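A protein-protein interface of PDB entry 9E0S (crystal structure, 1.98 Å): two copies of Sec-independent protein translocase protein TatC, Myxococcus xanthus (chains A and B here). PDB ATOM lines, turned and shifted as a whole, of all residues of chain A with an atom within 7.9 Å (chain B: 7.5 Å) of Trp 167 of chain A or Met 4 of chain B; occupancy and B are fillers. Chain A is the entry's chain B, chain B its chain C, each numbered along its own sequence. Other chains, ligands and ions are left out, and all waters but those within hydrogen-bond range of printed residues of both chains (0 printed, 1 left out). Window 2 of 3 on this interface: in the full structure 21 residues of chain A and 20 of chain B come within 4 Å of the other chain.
The backbone carbonyl oxygen (O) of Ser 3 of chain B is in hydrogen-bond range of the guanidinium group (NH2) of Arg 166 of chain A (3.0 Å).
OE2 of Glu 163 of chain A is in salt-bridge range of NH2 of Arg 166 of chain A (2.7 Å).
O of Met 4 of chain B lies within hydrogen-bond range of N of Met 174 of chain B (2.9 Å).
O of Thr 6 of chain B is in hydrogen-bond range of N of Leu 172 of chain B, at 2.9 Å.
Among the printed residues, pairs that only touch across the chains: Trp 167 of chain A with Ser 3 of chain B (3.95 Å), Trp 167 of chain A with Met 4 of chain B (3.5 Å), Trp 167 of chain A with Phe 5 of chain B (3.4 Å), Trp 167 of chain A with Thr 6 of chain B (3.4 Å), Met 171 of chain A with Leu 172 of chain B (3.5 Å) and Met 174 of chain A with Leu 172 of chain B (3.9 Å).
Of the printed residues of chain B, Arg 166 of chain A touches Ser 3 (2.3 Å).
Trp 167 of chain A touches four residues of chain B.
Printed residues of chain B within 4 Å of Met 171 of chain A: Leu 172 (3.5 Å).
Met 4 of chain B touches one residue of chain A.
Printed residues of chain A within 4 Å of Phe 5 of chain B: Trp 167 (3.4 Å).
Of the printed residues of chain A, Thr 6 of chain B touches Trp 167.
Printed residues of chain A within 4 Å of Leu 172 of chain B: Met 171 and Met 174.
The nearest residue of chain B that does not touch Trp 167 of chain A is Leu 172 of chain B (4.1 Å).
The nearest residue of chain A that does not touch Met 4 of chain B is Arg 166 of chain A (4.5 Å).
Of the 14 printed residues of chain A, 4 touch a printed residue of chain B.
Hydrophobic or aromatic side chains of chain A that line the printed part of chain B: Trp 167, Met 171 and Met 174.
Of the 15 printed residues of chain B, 5 touch a printed residue of chain A.
Among the printed residues, 7 pairs touch across the chains.
Among the printed residues, no Asp or Glu carboxylate lies within 4 Å of a Lys or Arg side-chain nitrogen of the other chain.
Met 171 of chain A touches Leu 172 of chain B, but with the chains exchanged Leu 172 of chain A does not touch Met 171 of chain B (12.9 Å).
Met 174 of chain A touches Leu 172 of chain B, but with the chains exchanged Leu 172 of chain A does not touch Met 174 of chain B (12.6 Å).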
ATOM      1  N   ALA A 161      -0.830 -10.552  -9.778  1.00  0.00           N
ATOM      2  CA  ALA A 161      -0.909 -12.008  -9.754  1.00  0.00           C
ATOM      3  C   ALA A 161      -1.908 -12.521 -10.784  1.00  0.00           C
ATOM      4  O   ALA A 161      -1.688 -13.565 -11.410  1.00  0.00           O
ATOM      5  CB  ALA A 161      -1.280 -12.491  -8.350  1.00  0.00           C
ATOM      6  N   HIS A 162      -3.012 -11.801 -10.979  1.00  0.00           N
ATOM      7  CA  HIS A 162      -3.996 -12.229 -11.962  1.00  0.00           C
ATOM      8  C   HIS A 162      -3.489 -12.007 -13.383  1.00  0.00           C
ATOM      9  O   HIS A 162      -3.727 -12.831 -14.273  1.00  0.00           O
ATOM     10  CB  HIS A 162      -5.303 -11.479 -11.742  1.00  0.00           C
ATOM     11  CG  HIS A 162      -6.275 -11.651 -12.858  1.00  0.00           C
ATOM     12  ND1 HIS A 162      -7.144 -12.717 -12.923  1.00  0.00           N
ATOM     13  CD2 HIS A 162      -6.502 -10.906 -13.966  1.00  0.00           C
ATOM     14  CE1 HIS A 162      -7.866 -12.621 -14.023  1.00  0.00           C
ATOM     15  NE2 HIS A 162      -7.500 -11.530 -14.670  1.00  0.00           N
ATOM     16  N   GLU A 163      -2.806 -10.888 -13.615  1.00  0.00           N
ATOM     17  CA  GLU A 163      -2.251 -10.619 -14.932  1.00  0.00           C
ATOM     18  C   GLU A 163      -1.122 -11.586 -15.253  1.00  0.00           C
ATOM     19  O   GLU A 163      -0.971 -12.006 -16.405  1.00  0.00           O
ATOM     20  CB  GLU A 163      -1.771  -9.174 -15.009  1.00  0.00           C
ATOM     21  CG  GLU A 163      -1.545  -8.695 -16.419  1.00  0.00           C
ATOM     22  CD  GLU A 163      -2.770  -8.882 -17.291  1.00  0.00           C
ATOM     23  OE1 GLU A 163      -3.902  -8.695 -16.789  1.00  0.00           O
ATOM     24  OE2 GLU A 163      -2.599  -9.229 -18.479  1.00  0.00           O
ATOM     25  N   ALA A 164      -0.341 -11.975 -14.243  1.00  0.00           N
ATOM     26  CA  ALA A 164       0.702 -12.974 -14.454  1.00  0.00           C
ATOM     27  C   ALA A 164       0.101 -14.327 -14.831  1.00  0.00           C
ATOM     28  O   ALA A 164       0.488 -14.934 -15.839  1.00  0.00           O
ATOM     29  CB  ALA A 164       1.563 -13.105 -13.201  1.00  0.00           C
ATOM     30  N   ALA A 165      -0.852 -14.811 -14.030  1.00  0.00           N
ATOM     31  CA  ALA A 165      -1.449 -16.125 -14.269  1.00  0.00           C
ATOM     32  C   ALA A 165      -2.256 -16.168 -15.563  1.00  0.00           C
ATOM     33  O   ALA A 165      -2.404 -17.239 -16.166  1.00  0.00           O
ATOM     34  CB  ALA A 165      -2.339 -16.523 -13.091  1.00  0.00           C
ATOM     35  N   ARG A 166      -2.787 -15.026 -16.002  1.00  0.00           N
ATOM     36  CA  ARG A 166      -3.591 -15.002 -17.220  1.00  0.00           C
ATOM     37  C   ARG A 166      -2.784 -15.477 -18.422  1.00  0.00           C
ATOM     38  O   ARG A 166      -3.314 -16.160 -19.305  1.00  0.00           O
ATOM     39  CB  ARG A 166      -4.126 -13.591 -17.463  1.00  0.00           C
ATOM     40  CG  ARG A 166      -5.375 -13.520 -18.298  1.00  0.00           C
ATOM     41  CD  ARG A 166      -6.015 -12.135 -18.190  1.00  0.00           C
ATOM     42  NE  ARG A 166      -5.154 -11.102 -18.750  1.00  0.00           N
ATOM     43  CZ  ARG A 166      -5.260 -10.626 -19.983  1.00  0.00           C
ATOM     44  NH1 ARG A 166      -6.213 -11.042 -20.802  1.00  0.00           N
ATOM     45  NH2 ARG A 166      -4.389  -9.711 -20.405  1.00  0.00           N
ATOM     46  N   TRP A 167      -1.501 -15.124 -18.477  1.00  0.00           N
ATOM     47  CA  TRP A 167      -0.648 -15.509 -19.590  1.00  0.00           C
ATOM     48  C   TRP A 167       0.303 -16.646 -19.257  1.00  0.00           C
ATOM     49  O   TRP A 167       0.755 -17.346 -20.173  1.00  0.00           O
ATOM     50  CB  TRP A 167       0.167 -14.315 -20.071  1.00  0.00           C
ATOM     51  CG  TRP A 167      -0.649 -13.286 -20.735  1.00  0.00           C
ATOM     52  CD1 TRP A 167      -1.032 -12.084 -20.219  1.00  0.00           C
ATOM     53  CD2 TRP A 167      -1.200 -13.358 -22.052  1.00  0.00           C
ATOM     54  NE1 TRP A 167      -1.783 -11.396 -21.141  1.00  0.00           N
ATOM     55  CE2 TRP A 167      -1.900 -12.158 -22.276  1.00  0.00           C
ATOM     56  CE3 TRP A 167      -1.167 -14.321 -23.065  1.00  0.00           C
ATOM     57  CZ2 TRP A 167      -2.553 -11.889 -23.476  1.00  0.00           C
ATOM     58  CZ3 TRP A 167      -1.824 -14.054 -24.260  1.00  0.00           C
ATOM     59  CH2 TRP A 167      -2.512 -12.849 -24.451  1.00  0.00           C
ATOM     60  N   THR A 168       0.623 -16.836 -17.981  1.00  0.00           N
ATOM     61  CA  THR A 168       1.494 -17.933 -17.604  1.00  0.00           C
ATOM     62  C   THR A 168       0.817 -19.273 -17.846  1.00  0.00           C
ATOM     63  O   THR A 168       1.448 -20.199 -18.366  1.00  0.00           O
ATOM     64  CB  THR A 168       1.924 -17.790 -16.138  1.00  0.00           C
ATOM     65  OG1 THR A 168       2.734 -16.619 -16.012  1.00  0.00           O
ATOM     66  CG2 THR A 168       2.740 -18.986 -15.704  1.00  0.00           C
ATOM     67  N   ARG A 169      -0.469 -19.396 -17.498  1.00  0.00           N
ATOM     68  CA  ARG A 169      -1.141 -20.680 -17.669  1.00  0.00           C
ATOM     69  C   ARG A 169      -1.137 -21.139 -19.124  1.00  0.00           C
ATOM     70  O   ARG A 169      -0.784 -22.302 -19.376  1.00  0.00           O
ATOM     71  CB  ARG A 169      -2.562 -20.620 -17.099  1.00  0.00           C
ATOM     72  CG  ARG A 169      -2.590 -20.447 -15.602  1.00  0.00           C
ATOM     73  CD  ARG A 169      -4.007 -20.406 -15.062  1.00  0.00           C
ATOM     74  NE  ARG A 169      -4.000 -20.074 -13.643  1.00  0.00           N
ATOM     75  CZ  ARG A 169      -3.698 -20.929 -12.674  1.00  0.00           C
ATOM     76  NH1 ARG A 169      -3.399 -22.194 -12.932  1.00  0.00           N
ATOM     77  NH2 ARG A 169      -3.695 -20.502 -11.414  1.00  0.00           N
ATOM     78  N   PRO A 170      -1.479 -20.307 -20.117  1.00  0.00           N
ATOM     79  CA  PRO A 170      -1.379 -20.796 -21.505  1.00  0.00           C
ATOM     80  C   PRO A 170       0.051 -20.990 -21.971  1.00  0.00           C
ATOM     81  O   PRO A 170       0.325 -21.935 -22.721  1.00  0.00           O
ATOM     82  CB  PRO A 170      -2.106 -19.713 -22.318  1.00  0.00           C
ATOM     83  CG  PRO A 170      -2.088 -18.510 -21.458  1.00  0.00           C
ATOM     84  CD  PRO A 170      -2.170 -19.005 -20.055  1.00  0.00           C
ATOM     85  N   MET A 171       0.979 -20.134 -21.555  1.00  0.00           N
ATOM     86  CA  MET A 171       2.370 -20.312 -21.970  1.00  0.00           C
ATOM     87  C   MET A 171       2.963 -21.612 -21.465  1.00  0.00           C
ATOM     88  O   MET A 171       3.757 -22.245 -22.168  1.00  0.00           O
ATOM     89  CB  MET A 171       3.232 -19.145 -21.497  1.00  0.00           C
ATOM     90  CG  MET A 171       2.978 -17.915 -22.298  1.00  0.00           C
ATOM     91  SD  MET A 171       3.947 -16.430 -21.544  1.00  0.00           S
ATOM     92  CE  MET A 171       5.599 -16.721 -22.410  1.00  0.00           C
ATOM     93  N   LEU A 172       2.572 -22.004 -20.248  1.00  0.00           N
ATOM     94  CA  LEU A 172       2.983 -23.301 -19.718  1.00  0.00           C
ATOM     95  C   LEU A 172       2.398 -24.440 -20.545  1.00  0.00           C
ATOM     96  O   LEU A 172       3.080 -25.436 -20.807  1.00  0.00           O
ATOM     97  CB  LEU A 172       2.560 -23.441 -18.253  1.00  0.00           C
ATOM     98  CG  LEU A 172       3.423 -22.695 -17.234  1.00  0.00           C
ATOM     99  CD1 LEU A 172       2.719 -22.588 -15.888  1.00  0.00           C
ATOM    100  CD2 LEU A 172       4.761 -23.400 -17.077  1.00  0.00           C
ATOM    101  N   SER A 173       1.129 -24.322 -20.942  1.00  0.00           N
ATOM    102  CA  SER A 173       0.514 -25.362 -21.758  1.00  0.00           C
ATOM    103  C   SER A 173       1.210 -25.489 -23.109  1.00  0.00           C
ATOM    104  O   SER A 173       1.462 -26.600 -23.585  1.00  0.00           O
ATOM    105  CB  SER A 173      -0.974 -25.065 -21.954  1.00  0.00           C
ATOM    106  OG  SER A 173      -1.660 -25.094 -20.724  1.00  0.00           O
ATOM    107  N   MET A 174       1.545 -24.368 -23.730  1.00  0.00           N
ATOM    108  CA  MET A 174       2.218 -24.374 -25.028  1.00  0.00           C
ATOM    109  C   MET A 174       3.618 -24.946 -24.907  1.00  0.00           C
ATOM    110  O   MET A 174       4.038 -25.779 -25.715  1.00  0.00           O
ATOM    111  CB  MET A 174       2.283 -22.960 -25.592  1.00  0.00           C
ATOM    112  CG  MET A 174       0.947 -22.464 -26.120  1.00  0.00           C
ATOM    113  SD  MET A 174       0.876 -20.529 -26.323  1.00  0.00           S
ATOM    114  CE  MET A 174       2.286 -20.212 -27.600  1.00  0.00           C
ATOM    115  N   GLY B   2      -2.894  -4.924 -25.399  1.00  0.00           N
ATOM    116  CA  GLY B   2      -4.001  -4.868 -24.465  1.00  0.00           C
ATOM    117  C   GLY B   2      -4.117  -6.111 -23.604  1.00  0.00           C
ATOM    118  O   GLY B   2      -3.111  -6.654 -23.142  1.00  0.00           O
ATOM    119  N   SER B   3      -5.350  -6.564 -23.383  1.00  0.00           N
ATOM    120  CA  SER B   3      -5.605  -7.748 -22.575  1.00  0.00           C
ATOM    121  C   SER B   3      -5.758  -9.011 -23.409  1.00  0.00           C
ATOM    122  O   SER B   3      -6.011 -10.077 -22.844  1.00  0.00           O
ATOM    123  CB  SER B   3      -6.857  -7.553 -21.710  1.00  0.00           C
ATOM    124  OG  SER B   3      -8.028  -7.465 -22.507  1.00  0.00           O
ATOM    125  N   MET B   4      -5.623  -8.916 -24.728  1.00  0.00           N
ATOM    126  CA  MET B   4      -5.751 -10.080 -25.604  1.00  0.00           C
ATOM    127  C   MET B   4      -4.437 -10.377 -26.318  1.00  0.00           C
ATOM    128  O   MET B   4      -4.327 -11.351 -27.064  1.00  0.00           O
ATOM    129  CB  MET B   4      -6.868  -9.862 -26.630  1.00  0.00           C
ATOM    130  CG  MET B   4      -8.233  -9.549 -26.015  1.00  0.00           C
ATOM    131  SD  MET B   4      -8.986 -11.019 -24.946  1.00  0.00           S
ATOM    132  CE  MET B   4      -9.519 -12.234 -26.389  1.00  0.00           C
ATOM    133  N   PHE B   5      -3.446  -9.515 -26.093  1.00  0.00           N
ATOM    134  CA  PHE B   5      -2.127  -9.636 -26.693  1.00  0.00           C
ATOM    135  C   PHE B   5      -1.088  -9.545 -25.587  1.00  0.00           C
ATOM    136  O   PHE B   5      -1.314  -8.898 -24.563  1.00  0.00           O
ATOM    137  CB  PHE B   5      -1.855  -8.522 -27.736  1.00  0.00           C
ATOM    138  CG  PHE B   5      -2.798  -8.533 -28.920  1.00  0.00           C
ATOM    139  CD1 PHE B   5      -4.118  -8.115 -28.786  1.00  0.00           C
ATOM    140  CD2 PHE B   5      -2.354  -8.931 -30.177  1.00  0.00           C
ATOM    141  CE1 PHE B   5      -4.985  -8.117 -29.880  1.00  0.00           C
ATOM    142  CE2 PHE B   5      -3.213  -8.930 -31.274  1.00  0.00           C
ATOM    143  CZ  PHE B   5      -4.530  -8.523 -31.124  1.00  0.00           C
ATOM    144  N   THR B   6       0.049 -10.206 -25.788  1.00  0.00           N
ATOM    145  CA  THR B   6       1.197  -9.997 -24.916  1.00  0.00           C
ATOM    146  C   THR B   6       2.461 -10.182 -25.735  1.00  0.00           C
ATOM    147  O   THR B   6       2.499 -10.969 -26.683  1.00  0.00           O
ATOM    148  CB  THR B   6       1.208 -10.937 -23.703  1.00  0.00           C
ATOM    149  OG1 THR B   6       2.299 -10.589 -22.840  1.00  0.00           O
ATOM    150  CG2 THR B   6       1.377 -12.364 -24.132  1.00  0.00           C
ATOM    151  N   PHE B   7       3.498  -9.447 -25.370  1.00  0.00           N
ATOM    152  CA  PHE B   7       4.721  -9.434 -26.150  1.00  0.00           C
ATOM    153  C   PHE B   7       5.824 -10.150 -25.400  1.00  0.00           C
ATOM    154  O   PHE B   7       6.045  -9.894 -24.213  1.00  0.00           O
ATOM    155  CB  PHE B   7       5.111  -8.006 -26.508  1.00  0.00           C
ATOM    156  CG  PHE B   7       4.296  -7.474 -27.617  1.00  0.00           C
ATOM    157  CD1 PHE B   7       3.078  -6.875 -27.365  1.00  0.00           C
ATOM    158  CD2 PHE B   7       4.694  -7.668 -28.926  1.00  0.00           C
ATOM    159  CE1 PHE B   7       2.295  -6.426 -28.400  1.00  0.00           C
ATOM    160  CE2 PHE B   7       3.922  -7.221 -29.963  1.00  0.00           C
ATOM    161  CZ  PHE B   7       2.715  -6.610 -29.702  1.00  0.00           C
ATOM    162  N   MET B 171       4.962 -12.302 -30.594  1.00  0.00           N
ATOM    163  CA  MET B 171       3.879 -12.046 -29.652  1.00  0.00           C
ATOM    164  C   MET B 171       2.858 -13.167 -29.574  1.00  0.00           C
ATOM    165  O   MET B 171       2.762 -14.017 -30.459  1.00  0.00           O
ATOM    166  CB  MET B 171       3.171 -10.740 -30.011  1.00  0.00           C
ATOM    167  CG  MET B 171       2.153 -10.862 -31.131  1.00  0.00           C
ATOM    168  SD  MET B 171       1.406  -9.132 -31.658  1.00  0.00           S
ATOM    169  CE  MET B 171       2.801  -8.590 -32.923  1.00  0.00           C
ATOM    170  N   LEU B 172       2.100 -13.169 -28.488  1.00  0.00           N
ATOM    171  CA  LEU B 172       1.030 -14.125 -28.278  1.00  0.00           C
ATOM    172  C   LEU B 172      -0.283 -13.375 -28.339  1.00  0.00           C
ATOM    173  O   LEU B 172      -0.365 -12.230 -27.894  1.00  0.00           O
ATOM    174  CB  LEU B 172       1.148 -14.826 -26.928  1.00  0.00           C
ATOM    175  CG  LEU B 172       2.526 -15.392 -26.622  1.00  0.00           C
ATOM    176  CD1 LEU B 172       2.499 -16.073 -25.283  1.00  0.00           C
ATOM    177  CD2 LEU B 172       2.944 -16.357 -27.710  1.00  0.00           C
ATOM    178  N   SER B 173      -1.305 -14.015 -28.888  1.00  0.00           N
ATOM    179  CA  SER B 173      -2.629 -13.419 -28.875  1.00  0.00           C
ATOM    180  C   SER B 173      -3.654 -14.500 -28.581  1.00  0.00           C
ATOM    181  O   SER B 173      -3.516 -15.640 -29.032  1.00  0.00           O
ATOM    182  CB  SER B 173      -2.938 -12.715 -30.198  1.00  0.00           C
ATOM    183  OG  SER B 173      -3.194 -13.661 -31.217  1.00  0.00           O
ATOM    184  N   MET B 174      -4.656 -14.143 -27.791  1.00  0.00           N
ATOM    185  CA  MET B 174      -5.795 -15.020 -27.578  1.00  0.00           C
ATOM    186  C   MET B 174      -6.923 -14.602 -28.530  1.00  0.00           C
ATOM    187  O   MET B 174      -7.192 -13.411 -28.705  1.00  0.00           O
ATOM    188  CB  MET B 174      -6.262 -14.965 -26.115  1.00  0.00           C
ATOM    189  CG  MET B 174      -7.288 -16.053 -25.766  1.00  0.00           C
ATOM    190  SD  MET B 174      -8.166 -15.844 -24.016  1.00  0.00           S
ATOM    191  CE  MET B 174      -7.027 -14.430 -23.277  1.00  0.00           C
ATOM    192  N   HIS B 175      -7.549 -15.580 -29.171  1.00  0.00           N
ATOM    193  CA  HIS B 175      -8.689 -15.323 -30.035  1.00  0.00           C
ATOM    194  C   HIS B 175      -9.960 -15.299 -29.204  1.00  0.00           C
ATOM    195  O   HIS B 175     -10.097 -16.050 -28.236  1.00  0.00           O
ATOM    196  CB  HIS B 175      -8.829 -16.402 -31.111  1.00  0.00           C
ATOM    197  CG  HIS B 175      -7.717 -16.429 -32.108  1.00  0.00           C
ATOM    198  ND1 HIS B 175      -6.397 -16.593 -31.751  1.00  0.00           N
ATOM    199  CD2 HIS B 175      -7.735 -16.344 -33.459  1.00  0.00           C
ATOM    200  CE1 HIS B 175      -5.648 -16.594 -32.837  1.00  0.00           C
ATOM    201  NE2 HIS B 175      -6.436 -16.447 -33.888  1.00  0.00           N
ATOM    202  N   GLU B 176     -10.901 -14.445 -29.600  1.00  0.00           N
ATOM    203  CA  GLU B 176     -12.221 -14.465 -28.984  1.00  0.00           C
ATOM    204  C   GLU B 176     -13.058 -15.570 -29.617  1.00  0.00           C
ATOM    205  O   GLU B 176     -13.185 -15.644 -30.842  1.00  0.00           O
ATOM    206  CB  GLU B 176     -12.927 -13.116 -29.129  1.00  0.00           C
ATOM    207  CG  GLU B 176     -12.041 -11.917 -28.875  1.00  0.00           C
ATOM    208  CD  GLU B 176     -12.831 -10.641 -28.665  1.00  0.00           C
ATOM    209  OE1 GLU B 176     -13.990 -10.727 -28.202  1.00  0.00           O
ATOM    210  OE2 GLU B 176     -12.293  -9.556 -28.966  1.00  0.00           O
ATOM    211  N   GLN B 177     -13.622 -16.434 -28.788  1.00  0.00           N
ATOM    212  CA  GLN B 177     -14.483 -17.496 -29.286  1.00  0.00           C
ATOM    213  C   GLN B 177     -15.881 -16.935 -29.527  1.00  0.00           C
ATOM    214  O   GLN B 177     -16.552 -16.502 -28.587  1.00  0.00           O
ATOM    215  CB  GLN B 177     -14.508 -18.650 -28.295  1.00  0.00           C
ATOM    216  CG  GLN B 177     -15.425 -19.780 -28.686  1.00  0.00           C
ATOM    217  CD  GLN B 177     -14.993 -21.110 -28.092  1.00  0.00           C
ATOM    218  OE1 GLN B 177     -14.320 -21.156 -27.061  1.00  0.00           O
ATOM    219  NE2 GLN B 177     -15.370 -22.200 -28.750  1.00  0.00           N
ATOM    220  N   PHE B 184     -12.347 -15.030 -33.443  1.00  0.00           N
ATOM    221  CA  PHE B 184     -11.871 -13.764 -33.988  1.00  0.00           C
ATOM    222  C   PHE B 184     -10.553 -13.366 -33.346  1.00  0.00           C
ATOM    223  O   PHE B 184     -10.328 -13.611 -32.158  1.00  0.00           O
ATOM    224  CB  PHE B 184     -12.869 -12.605 -33.773  1.00  0.00           C
ATOM    225  CG  PHE B 184     -12.269 -11.227 -34.039  1.00  0.00           C
ATOM    226  CD1 PHE B 184     -11.605 -10.521 -33.033  1.00  0.00           C
ATOM    227  CD2 PHE B 184     -12.358 -10.650 -35.295  1.00  0.00           C
ATOM    228  CE1 PHE B 184     -11.037  -9.278 -33.281  1.00  0.00           C
ATOM    229  CE2 PHE B 184     -11.801  -9.400 -35.546  1.00  0.00           C
ATOM    230  CZ  PHE B 184     -11.140  -8.714 -34.536  1.00  0.00           C
ATOM    231  N   GLN B 185      -9.704 -12.702 -34.129  1.00  0.00           N
ATOM    232  CA  GLN B 185      -8.556 -11.986 -33.581  1.00  0.00           C
ATOM    233  C   GLN B 185      -8.110 -10.902 -34.548  1.00  0.00           C
ATOM    234  O   GLN B 185      -8.616 -10.825 -35.667  1.00  0.00           O
ATOM    235  CB  GLN B 185      -7.399 -12.931 -33.282  1.00  0.00           C
ATOM    236  CG  GLN B 185      -6.444 -13.130 -34.431  1.00  0.00           C
ATOM    237  CD  GLN B 185      -5.007 -13.003 -33.983  1.00  0.00           C
ATOM    238  OE1 GLN B 185      -4.689 -12.173 -33.130  1.00  0.00           O
ATOM    239  NE2 GLN B 185      -4.128 -13.834 -34.544  1.00  0.00           N
